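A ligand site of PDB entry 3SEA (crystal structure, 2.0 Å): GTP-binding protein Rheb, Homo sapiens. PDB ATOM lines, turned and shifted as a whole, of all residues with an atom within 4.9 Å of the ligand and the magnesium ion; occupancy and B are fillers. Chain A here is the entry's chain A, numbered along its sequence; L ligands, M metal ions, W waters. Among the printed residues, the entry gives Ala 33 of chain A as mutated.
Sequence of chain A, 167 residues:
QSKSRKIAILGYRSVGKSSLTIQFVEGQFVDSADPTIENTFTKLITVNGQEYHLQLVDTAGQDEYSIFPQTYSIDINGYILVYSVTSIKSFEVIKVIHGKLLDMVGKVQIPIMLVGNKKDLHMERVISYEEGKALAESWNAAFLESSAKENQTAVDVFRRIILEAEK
OD1 of Asp 58 is in hydrogen-bond range of N of Ser 18, at 3.5 Å.
O of Val 30 lies within hydrogen-bond range of OG of Ser 19 (3.3 Å).
The side-chain amino group (NZ) of Lys 17 lies within hydrogen-bond range of the backbone carbonyl oxygen (O) of Tyr 12.
OG of Ser 147 lies within hydrogen-bond range of OD1 of Asp 120 (2.8 Å).
O of Ser 14 sits at hydrogen-bond distance from NZ of Lys 118, 2.8 Å away.
The side-chain amide oxygen (OD1) of Asn 117 lies within hydrogen-bond range of the side-chain hydroxyl (OG) of Ser 146, at 2.8 Å.
The backbone carbonyl oxygen (O) of Ser 146 lies within hydrogen-bond range of the backbone NH (N) of Lys 118 (3.0 Å).
The backbone NH of Lys 149 lies close to the side-chain hydroxyl of Ser 147.
N of Ser 18 is in hydrogen-bond range of O6 of the ligand.
The backbone carbonyl oxygen (O) of Asp 31 lies within hydrogen-bond range of an oxygen (O9) of the ligand, 2.5 Å away.
An oxygen (O10) of the ligand lies within hydrogen-bond range of the backbone carbonyl oxygen of Val 30.
N of Lys 17 sits at hydrogen-bond distance from O2 of the ligand, at 2.9 Å.
The side-chain amino group (NZ) of Lys 17 lies within salt-bridge range of an oxygen (O2) of the ligand (2.7 Å).
N4 of the ligand lies within hydrogen-bond range of OD2 of Asp 120 (2.7 Å).
The backbone NH of Ser 14 sits at hydrogen-bond distance from an oxygen (O1) of the ligand (2.7 Å).
O11 of the ligand is in hydrogen-bond range of N of Ala 148 (2.8 Å).
An oxygen (O6) of the ligand sits at hydrogen-bond distance from the backbone NH (N) of Ser 19.
An oxygen (O6) of the ligand lies within hydrogen-bond range of the side-chain hydroxyl (OG) of Ser 19 (2.9 Å).
An oxygen (O4) of the ligand sits at hydrogen-bond distance from the backbone NH of Gly 16.
ND2 of Asn 117 lies within hydrogen-bond range of N2 of the ligand (3.0 Å).
O11 of the ligand sits close to N of Lys 118 (3.4 Å).
The side-chain amino group (NZ) of Lys 118 lies within hydrogen-bond range of an oxygen (O8) of the ligand (3.3 Å).
N of Val 15 sits at hydrogen-bond distance from O2 of the ligand (3.3 Å).
Tyr 12 touches the ligand.
Arg 13 touches the ligand (C to O1, 3.8 Å).
Phe 29 touches the ligand (CZ to O10, 3.3 Å).
Leu 121 touches the ligand.
Ser 147 touches the ligand (CA to O11, 3.4 Å).
Lys 149 touches the ligand (CE to N4, 3.7 Å).
Water W7 is bound to the magnesium ion (2.1 Å).
Water W6 is bound to the magnesium ion, at 2.1 Å.
OG of Ser 18 is bound to the magnesium ion (2.1 Å).
Water W4 binds the magnesium ion, 2.2 Å away.
The magnesium ion is bound by O3 of the ligand.
Water W10 is bound to the magnesium ion (2.4 Å).
The magnesium ion has six donor atoms within binding distance.
Water W10 lies within hydrogen-bond range of O1 of the ligand and O of Pro 35.
Water W6 lies within hydrogen-bond range of the backbone carbonyl oxygen of Thr 59 (2.6 Å) and the side-chain carboxylate of Asp 58 (2.6 Å).
Water W5 bridges O5 of the ligand (2.5 Å) and N of Ala 33 (3.2 Å).
Water W3 lies within hydrogen-bond range of an oxygen (O1) of the ligand (2.7 Å) and the side-chain hydroxyl of Ser 14 (3.4 Å).
Water W1 bridges OD2 of Asp 31 (2.9 Å) and O10 of the ligand (2.9 Å).
Water W8 lies within hydrogen-bond range of NZ of Lys 118 (2.9 Å) and O8 of the ligand (3.3 Å).
Asp 58 touches the magnesium ion (OD2 to MG, 3.9 Å).
Two residues have an atom within 4 Å of the magnesium ion: Ser 18 and Asp 58.
Along chain A the residues within 4 Å of the magnesium ion span positions 18 to 58.
The nearest printed residue that does not touch the magnesium ion is Asp 34 (4.2 Å).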
ATOM      1  N   TYR A  12       8.957  22.199   7.569  1.00  0.00           N
ATOM      2  CA  TYR A  12       9.161  22.200   6.123  1.00  0.00           C
ATOM      3  C   TYR A  12       7.832  22.024   5.377  1.00  0.00           C
ATOM      4  O   TYR A  12       6.853  21.532   5.943  1.00  0.00           O
ATOM      5  CB  TYR A  12      10.119  21.061   5.784  1.00  0.00           C
ATOM      6  CG  TYR A  12      10.525  20.958   4.334  1.00  0.00           C
ATOM      7  CD1 TYR A  12      11.255  21.974   3.716  1.00  0.00           C
ATOM      8  CD2 TYR A  12      10.205  19.816   3.581  1.00  0.00           C
ATOM      9  CE1 TYR A  12      11.649  21.873   2.385  1.00  0.00           C
ATOM     10  CE2 TYR A  12      10.602  19.698   2.251  1.00  0.00           C
ATOM     11  CZ  TYR A  12      11.320  20.735   1.664  1.00  0.00           C
ATOM     12  OH  TYR A  12      11.714  20.640   0.355  1.00  0.00           O
ATOM     13  N   ARG A  13       7.794  22.416   4.108  1.00  0.00           N
ATOM     14  CA  ARG A  13       6.586  22.278   3.308  1.00  0.00           C
ATOM     15  C   ARG A  13       6.115  20.816   3.200  1.00  0.00           C
ATOM     16  O   ARG A  13       6.938  19.892   3.145  1.00  0.00           O
ATOM     17  CB  ARG A  13       6.782  22.890   1.908  1.00  0.00           C
ATOM     18  CG  ARG A  13       8.159  22.660   1.317  1.00  0.00           C
ATOM     19  CD  ARG A  13       8.459  23.641   0.167  1.00  0.00           C
ATOM     20  NE  ARG A  13       9.873  23.636  -0.206  1.00  0.00           N
ATOM     21  CZ  ARG A  13      10.758  24.550   0.197  1.00  0.00           C
ATOM     22  NH1 ARG A  13      10.379  25.537   0.984  1.00  0.00           N
ATOM     23  NH2 ARG A  13      12.019  24.463  -0.193  1.00  0.00           N
ATOM     24  N   SER A  14       4.797  20.637   3.203  1.00  0.00           N
ATOM     25  CA  SER A  14       4.168  19.327   3.021  1.00  0.00           C
ATOM     26  C   SER A  14       4.293  18.290   4.146  1.00  0.00           C
ATOM     27  O   SER A  14       3.927  17.132   3.953  1.00  0.00           O
ATOM     28  CB  SER A  14       4.671  18.694   1.720  1.00  0.00           C
ATOM     29  OG  SER A  14       4.317  19.503   0.608  1.00  0.00           O
ATOM     30  N   VAL A  15       4.802  18.666   5.314  1.00  0.00           N
ATOM     31  CA  VAL A  15       4.940  17.707   6.404  1.00  0.00           C
ATOM     32  C   VAL A  15       3.590  17.431   7.088  1.00  0.00           C
ATOM     33  O   VAL A  15       3.474  16.461   7.848  1.00  0.00           O
ATOM     34  CB  VAL A  15       5.952  18.163   7.486  1.00  0.00           C
ATOM     35  CG1 VAL A  15       7.330  18.372   6.869  1.00  0.00           C
ATOM     36  CG2 VAL A  15       5.456  19.425   8.223  1.00  0.00           C
ATOM     37  N   GLY A  16       2.609  18.288   6.849  1.00  0.00           N
ATOM     38  CA  GLY A  16       1.290  18.146   7.456  1.00  0.00           C
ATOM     39  C   GLY A  16       0.930  19.132   8.567  1.00  0.00           C
ATOM     40  O   GLY A  16       0.059  18.851   9.400  1.00  0.00           O
ATOM     41  N   LYS A  17       1.592  20.291   8.583  1.00  0.00           N
ATOM     42  CA  LYS A  17       1.256  21.329   9.555  1.00  0.00           C
ATOM     43  C   LYS A  17      -0.223  21.669   9.455  1.00  0.00           C
ATOM     44  O   LYS A  17      -0.949  21.636  10.457  1.00  0.00           O
ATOM     45  CB  LYS A  17       2.086  22.605   9.307  1.00  0.00           C
ATOM     46  CG  LYS A  17       3.597  22.385   9.491  1.00  0.00           C
ATOM     47  CD  LYS A  17       4.405  23.682   9.234  1.00  0.00           C
ATOM     48  CE  LYS A  17       4.162  24.244   7.837  1.00  0.00           C
ATOM     49  NZ  LYS A  17       4.754  23.375   6.788  1.00  0.00           N
ATOM     50  N   SER A  18      -0.671  21.986   8.255  1.00  0.00           N
ATOM     51  CA  SER A  18      -2.076  22.340   8.048  1.00  0.00           C
ATOM     52  C   SER A  18      -3.032  21.184   8.332  1.00  0.00           C
ATOM     53  O   SER A  18      -4.042  21.362   9.022  1.00  0.00           O
ATOM     54  CB  SER A  18      -2.297  22.876   6.639  1.00  0.00           C
ATOM     55  OG  SER A  18      -1.673  24.131   6.502  1.00  0.00           O
ATOM     56  N   SER A  19      -2.714  20.002   7.813  1.00  0.00           N
ATOM     57  CA  SER A  19      -3.610  18.868   7.980  1.00  0.00           C
ATOM     58  C   SER A  19      -3.764  18.524   9.457  1.00  0.00           C
ATOM     59  O   SER A  19      -4.865  18.260   9.940  1.00  0.00           O
ATOM     60  CB  SER A  19      -3.126  17.646   7.186  1.00  0.00           C
ATOM     61  OG  SER A  19      -3.122  17.889   5.793  1.00  0.00           O
ATOM     62  N   PHE A  29      -9.772  15.279   7.949  1.00  0.00           N
ATOM     63  CA  PHE A  29      -8.498  15.158   7.272  1.00  0.00           C
ATOM     64  C   PHE A  29      -8.616  15.768   5.879  1.00  0.00           C
ATOM     65  O   PHE A  29      -9.482  15.395   5.101  1.00  0.00           O
ATOM     66  CB  PHE A  29      -8.045  13.687   7.185  1.00  0.00           C
ATOM     67  CG  PHE A  29      -6.833  13.495   6.343  1.00  0.00           C
ATOM     68  CD1 PHE A  29      -5.596  13.947   6.770  1.00  0.00           C
ATOM     69  CD2 PHE A  29      -6.925  12.909   5.096  1.00  0.00           C
ATOM     70  CE1 PHE A  29      -4.479  13.781   5.988  1.00  0.00           C
ATOM     71  CE2 PHE A  29      -5.797  12.756   4.296  1.00  0.00           C
ATOM     72  CZ  PHE A  29      -4.571  13.183   4.749  1.00  0.00           C
ATOM     73  N   VAL A  30      -7.736  16.715   5.553  1.00  0.00           N
ATOM     74  CA  VAL A  30      -7.791  17.293   4.218  1.00  0.00           C
ATOM     75  C   VAL A  30      -6.602  16.882   3.335  1.00  0.00           C
ATOM     76  O   VAL A  30      -5.497  16.630   3.813  1.00  0.00           O
ATOM     77  CB  VAL A  30      -7.952  18.816   4.244  1.00  0.00           C
ATOM     78  CG1 VAL A  30      -9.130  19.188   5.132  1.00  0.00           C
ATOM     79  CG2 VAL A  30      -6.666  19.492   4.719  1.00  0.00           C
ATOM     80  N   ASP A  31      -6.877  16.800   2.050  1.00  0.00           N
ATOM     81  CA  ASP A  31      -5.898  16.305   1.091  1.00  0.00           C
ATOM     82  C   ASP A  31      -4.984  17.406   0.563  1.00  0.00           C
ATOM     83  O   ASP A  31      -3.946  17.125  -0.036  1.00  0.00           O
ATOM     84  CB  ASP A  31      -6.615  15.581  -0.052  1.00  0.00           C
ATOM     85  CG  ASP A  31      -7.260  14.294   0.412  1.00  0.00           C
ATOM     86  OD1 ASP A  31      -8.507  14.224   0.496  1.00  0.00           O
ATOM     87  OD2 ASP A  31      -6.505  13.354   0.733  1.00  0.00           O
ATOM     88  N   SER A  32      -5.357  18.665   0.795  1.00  0.00           N
ATOM     89  CA  SER A  32      -4.493  19.797   0.454  1.00  0.00           C
ATOM     90  C   SER A  32      -4.938  21.097   1.149  1.00  0.00           C
ATOM     91  O   SER A  32      -6.106  21.239   1.500  1.00  0.00           O
ATOM     92  CB  SER A  32      -4.446  19.990  -1.065  1.00  0.00           C
ATOM     93  OG  SER A  32      -5.643  20.596  -1.536  1.00  0.00           O
ATOM     94  N   ALA A  33      -3.998  22.034   1.267  1.00  0.00           N
ATOM     95  CA  ALA A  33      -4.262  23.376   1.776  1.00  0.00           C
ATOM     96  C   ALA A  33      -3.218  24.374   1.240  1.00  0.00           C
ATOM     97  O   ALA A  33      -2.046  24.031   1.111  1.00  0.00           O
ATOM     98  CB  ALA A  33      -4.271  23.387   3.289  1.00  0.00           C
ATOM     99  N   ASP A  34      -3.648  25.598   0.932  1.00  0.00           N
ATOM    100  CA  ASP A  34      -2.749  26.638   0.439  1.00  0.00           C
ATOM    101  C   ASP A  34      -1.376  26.541   1.093  1.00  0.00           C
ATOM    102  O   ASP A  34      -1.239  26.790   2.278  1.00  0.00           O
ATOM    103  CB  ASP A  34      -3.344  28.026   0.702  1.00  0.00           C
ATOM    104  CG  ASP A  34      -4.531  28.342  -0.202  1.00  0.00           C
ATOM    105  OD1 ASP A  34      -4.382  28.255  -1.434  1.00  0.00           O
ATOM    106  OD2 ASP A  34      -5.603  28.683   0.332  1.00  0.00           O
ATOM    107  N   PRO A  35      -0.360  26.201   0.311  1.00  0.00           N
ATOM    108  CA  PRO A  35       0.954  25.886   0.898  1.00  0.00           C
ATOM    109  C   PRO A  35       1.668  27.175   1.364  1.00  0.00           C
ATOM    110  O   PRO A  35       2.546  27.087   2.238  1.00  0.00           O
ATOM    111  CB  PRO A  35       1.721  25.221  -0.244  1.00  0.00           C
ATOM    112  CG  PRO A  35       1.017  25.663  -1.499  1.00  0.00           C
ATOM    113  CD  PRO A  35      -0.433  25.791  -1.120  1.00  0.00           C
ATOM    114  N   ASP A  58      -0.803  28.382  12.081  1.00  0.00           N
ATOM    115  CA  ASP A  58      -0.344  27.410  11.113  1.00  0.00           C
ATOM    116  C   ASP A  58       0.514  28.136  10.068  1.00  0.00           C
ATOM    117  O   ASP A  58      -0.012  28.630   9.073  1.00  0.00           O
ATOM    118  CB  ASP A  58      -1.564  26.770  10.438  1.00  0.00           C
ATOM    119  CG  ASP A  58      -1.191  25.852   9.300  1.00  0.00           C
ATOM    120  OD1 ASP A  58      -0.098  25.236   9.359  1.00  0.00           O
ATOM    121  OD2 ASP A  58      -1.985  25.732   8.344  1.00  0.00           O
ATOM    122  N   THR A  59       1.814  28.215  10.313  1.00  0.00           N
ATOM    123  CA  THR A  59       2.685  28.988   9.432  1.00  0.00           C
ATOM    124  C   THR A  59       2.779  28.327   8.067  1.00  0.00           C
ATOM    125  O   THR A  59       2.579  27.124   7.942  1.00  0.00           O
ATOM    126  CB  THR A  59       4.102  29.167  10.046  1.00  0.00           C
ATOM    127  OG1 THR A  59       4.808  27.921  10.021  1.00  0.00           O
ATOM    128  CG2 THR A  59       3.971  29.652  11.476  1.00  0.00           C
ATOM    129  N   ASN A 117       5.180  13.410  11.882  1.00  0.00           N
ATOM    130  CA  ASN A 117       3.850  13.231  11.326  1.00  0.00           C
ATOM    131  C   ASN A 117       3.828  12.204  10.196  1.00  0.00           C
ATOM    132  O   ASN A 117       4.870  11.764   9.716  1.00  0.00           O
ATOM    133  CB  ASN A 117       3.274  14.580  10.841  1.00  0.00           C
ATOM    134  CG  ASN A 117       1.802  14.488  10.450  1.00  0.00           C
ATOM    135  OD1 ASN A 117       0.986  13.890  11.175  1.00  0.00           O
ATOM    136  ND2 ASN A 117       1.454  15.048   9.292  1.00  0.00           N
ATOM    137  N   LYS A 118       2.615  11.843   9.768  1.00  0.00           N
ATOM    138  CA  LYS A 118       2.391  10.837   8.711  1.00  0.00           C
ATOM    139  C   LYS A 118       2.751   9.425   9.128  1.00  0.00           C
ATOM    140  O   LYS A 118       3.097   8.603   8.294  1.00  0.00           O
ATOM    141  CB  LYS A 118       3.116  11.219   7.401  1.00  0.00           C
ATOM    142  CG  LYS A 118       2.751  12.613   6.906  1.00  0.00           C
ATOM    143  CD  LYS A 118       3.191  12.837   5.454  1.00  0.00           C
ATOM    144  CE  LYS A 118       2.919  14.280   4.999  1.00  0.00           C
ATOM    145  NZ  LYS A 118       3.294  14.482   3.549  1.00  0.00           N
ATOM    146  N   LYS A 119       2.616   9.111  10.417  1.00  0.00           N
ATOM    147  CA  LYS A 119       2.962   7.767  10.873  1.00  0.00           C
ATOM    148  C   LYS A 119       2.091   6.661  10.237  1.00  0.00           C
ATOM    149  O   LYS A 119       2.461   5.496  10.281  1.00  0.00           O
ATOM    150  CB  LYS A 119       2.922   7.656  12.403  1.00  0.00           C
ATOM    151  CG  LYS A 119       1.519   7.577  12.987  1.00  0.00           C
ATOM    152  CD  LYS A 119       1.568   7.545  14.500  1.00  0.00           C
ATOM    153  CE  LYS A 119       0.207   7.244  15.108  1.00  0.00           C
ATOM    154  NZ  LYS A 119      -0.237   5.837  14.823  1.00  0.00           N
ATOM    155  N   ASP A 120       0.950   7.025   9.671  1.00  0.00           N
ATOM    156  CA  ASP A 120       0.087   6.055   8.986  1.00  0.00           C
ATOM    157  C   ASP A 120       0.698   5.544   7.684  1.00  0.00           C
ATOM    158  O   ASP A 120       0.274   4.499   7.167  1.00  0.00           O
ATOM    159  CB  ASP A 120      -1.265   6.675   8.687  1.00  0.00           C
ATOM    160  CG  ASP A 120      -1.146   7.904   7.831  1.00  0.00           C
ATOM    161  OD1 ASP A 120      -0.672   8.933   8.365  1.00  0.00           O
ATOM    162  OD2 ASP A 120      -1.496   7.851   6.637  1.00  0.00           O
ATOM    163  N   LEU A 121       1.664   6.273   7.144  1.00  0.00           N
ATOM    164  CA  LEU A 121       2.273   5.860   5.876  1.00  0.00           C
ATOM    165  C   LEU A 121       3.459   4.952   6.152  1.00  0.00           C
ATOM    166  O   LEU A 121       4.604   5.273   5.825  1.00  0.00           O
ATOM    167  CB  LEU A 121       2.709   7.072   5.065  1.00  0.00           C
ATOM    168  CG  LEU A 121       1.568   7.990   4.624  1.00  0.00           C
ATOM    169  CD1 LEU A 121       2.119   9.174   3.814  1.00  0.00           C
ATOM    170  CD2 LEU A 121       0.523   7.181   3.814  1.00  0.00           C
ATOM    171  N   SER A 146       2.499  11.373  14.982  1.00  0.00           N
ATOM    172  CA  SER A 146       1.107  11.659  14.736  1.00  0.00           C
ATOM    173  C   SER A 146       0.705  11.256  13.338  1.00  0.00           C
ATOM    174  O   SER A 146       1.560  10.985  12.485  1.00  0.00           O
ATOM    175  CB  SER A 146       0.837  13.169  14.893  1.00  0.00           C
ATOM    176  OG  SER A 146       1.559  13.914  13.896  1.00  0.00           O
ATOM    177  N   SER A 147      -0.598  11.257  13.113  1.00  0.00           N
ATOM    178  CA  SER A 147      -1.167  11.195  11.778  1.00  0.00           C
ATOM    179  C   SER A 147      -2.364  12.116  11.716  1.00  0.00           C
ATOM    180  O   SER A 147      -3.281  12.021  12.534  1.00  0.00           O
ATOM    181  CB  SER A 147      -1.655   9.776  11.447  1.00  0.00           C
ATOM    182  OG  SER A 147      -2.458   9.810  10.285  1.00  0.00           O
ATOM    183  N   ALA A 148      -2.361  12.990  10.724  1.00  0.00           N
ATOM    184  CA  ALA A 148      -3.471  13.926  10.559  1.00  0.00           C
ATOM    185  C   ALA A 148      -4.775  13.223  10.184  1.00  0.00           C
ATOM    186  O   ALA A 148      -5.844  13.835  10.199  1.00  0.00           O
ATOM    187  CB  ALA A 148      -3.127  14.982   9.527  1.00  0.00           C
ATOM    188  N   LYS A 149      -4.697  11.931   9.860  1.00  0.00           N
ATOM    189  CA  LYS A 149      -5.903  11.130   9.586  1.00  0.00           C
ATOM    190  C   LYS A 149      -6.548  10.649  10.878  1.00  0.00           C
ATOM    191  O   LYS A 149      -7.667  10.138  10.874  1.00  0.00           O
ATOM    192  CB  LYS A 149      -5.570   9.909   8.722  1.00  0.00           C
ATOM    193  CG  LYS A 149      -5.223  10.217   7.291  1.00  0.00           C
ATOM    194  CD  LYS A 149      -5.136   8.940   6.482  1.00  0.00           C
ATOM    195  CE  LYS A 149      -4.947   9.248   5.004  1.00  0.00           C
ATOM    196  NZ  LYS A 149      -4.748   8.006   4.203  1.00  0.00           N
HETATM  197  P1  LIG L   1       2.050  21.556   5.241  1.00  0.00           P
HETATM  198  O1  LIG L   1       2.668  22.178   3.997  1.00  0.00           O
HETATM  199  O2  LIG L   1       3.091  21.327   6.296  1.00  0.00           O
HETATM  200  O3  LIG L   1       0.934  22.363   5.840  1.00  0.00           O
HETATM  201  O4  LIG L   1       1.457  20.092   4.835  1.00  0.00           O
HETATM  202  P2  LIG L   1      -0.080  19.803   4.436  1.00  0.00           P
HETATM  203  O5  LIG L   1      -0.556  20.797   3.395  1.00  0.00           O
HETATM  204  O6  LIG L   1      -0.946  19.827   5.662  1.00  0.00           O
HETATM  205  O7  LIG L   1       0.014  18.319   3.843  1.00  0.00           O
HETATM  206  C1  LIG L   1       0.659  18.051   2.606  1.00  0.00           C
HETATM  207  C2  LIG L   1       0.081  16.755   2.083  1.00  0.00           C
HETATM  208  O8  LIG L   1       0.304  15.718   3.044  1.00  0.00           O
HETATM  209  C3  LIG L   1      -1.430  16.869   1.930  1.00  0.00           C
HETATM  210  O9  LIG L   1      -1.797  16.159   0.749  1.00  0.00           O
HETATM  211  C4  LIG L   1      -2.003  16.144   3.122  1.00  0.00           C
HETATM  212  O10 LIG L   1      -3.278  15.543   2.854  1.00  0.00           O
HETATM  213  C5  LIG L   1      -0.936  15.095   3.395  1.00  0.00           C
HETATM  214  N1  LIG L   1      -0.824  14.729   4.813  1.00  0.00           N
HETATM  215  C6  LIG L   1      -0.588  15.568   5.834  1.00  0.00           C
HETATM  216  N2  LIG L   1      -0.521  14.889   7.001  1.00  0.00           N
HETATM  217  C7  LIG L   1      -0.684  13.589   6.716  1.00  0.00           C
HETATM  218  C8  LIG L   1      -0.714  12.346   7.476  1.00  0.00           C
HETATM  219  O11 LIG L   1      -0.549  12.376   8.703  1.00  0.00           O
HETATM  220  N3  LIG L   1      -0.924  11.190   6.813  1.00  0.00           N
HETATM  221  C9  LIG L   1      -1.102  11.142   5.480  1.00  0.00           C
HETATM  222  N4  LIG L   1      -1.306   9.939   4.875  1.00  0.00           N
HETATM  223  N5  LIG L   1      -1.080  12.261   4.711  1.00  0.00           N
HETATM  224  C10 LIG L   1      -0.878  13.481   5.265  1.00  0.00           C
HETATM  225 MG    MG M   1       0.111  24.370   5.380  1.00  0.00          MG
HETATM  226  O   HOH W   1      -3.656  13.392   0.958  1.00  0.00           O
HETATM  227  O   HOH W   2      -2.026   9.614   1.994  1.00  0.00           O
HETATM  228  O   HOH W   3       1.919  21.710   1.425  1.00  0.00           O
HETATM  229  O   HOH W   4      -0.628  23.419   3.547  1.00  0.00           O
HETATM  230  O   HOH W   5      -1.180  20.585   0.953  1.00  0.00           O
HETATM  231  O   HOH W   6       1.027  25.275   7.008  1.00  0.00           O
HETATM  232  O   HOH W   7      -0.512  26.240   4.734  1.00  0.00           O
HETATM  233  O   HOH W   8       1.358  12.647   2.420  1.00  0.00           O
HETATM  234  O   HOH W   9       0.140  14.054   0.090  1.00  0.00           O
HETATM  235  O   HOH W  10       2.166  24.874   4.161  1.00  0.00           O
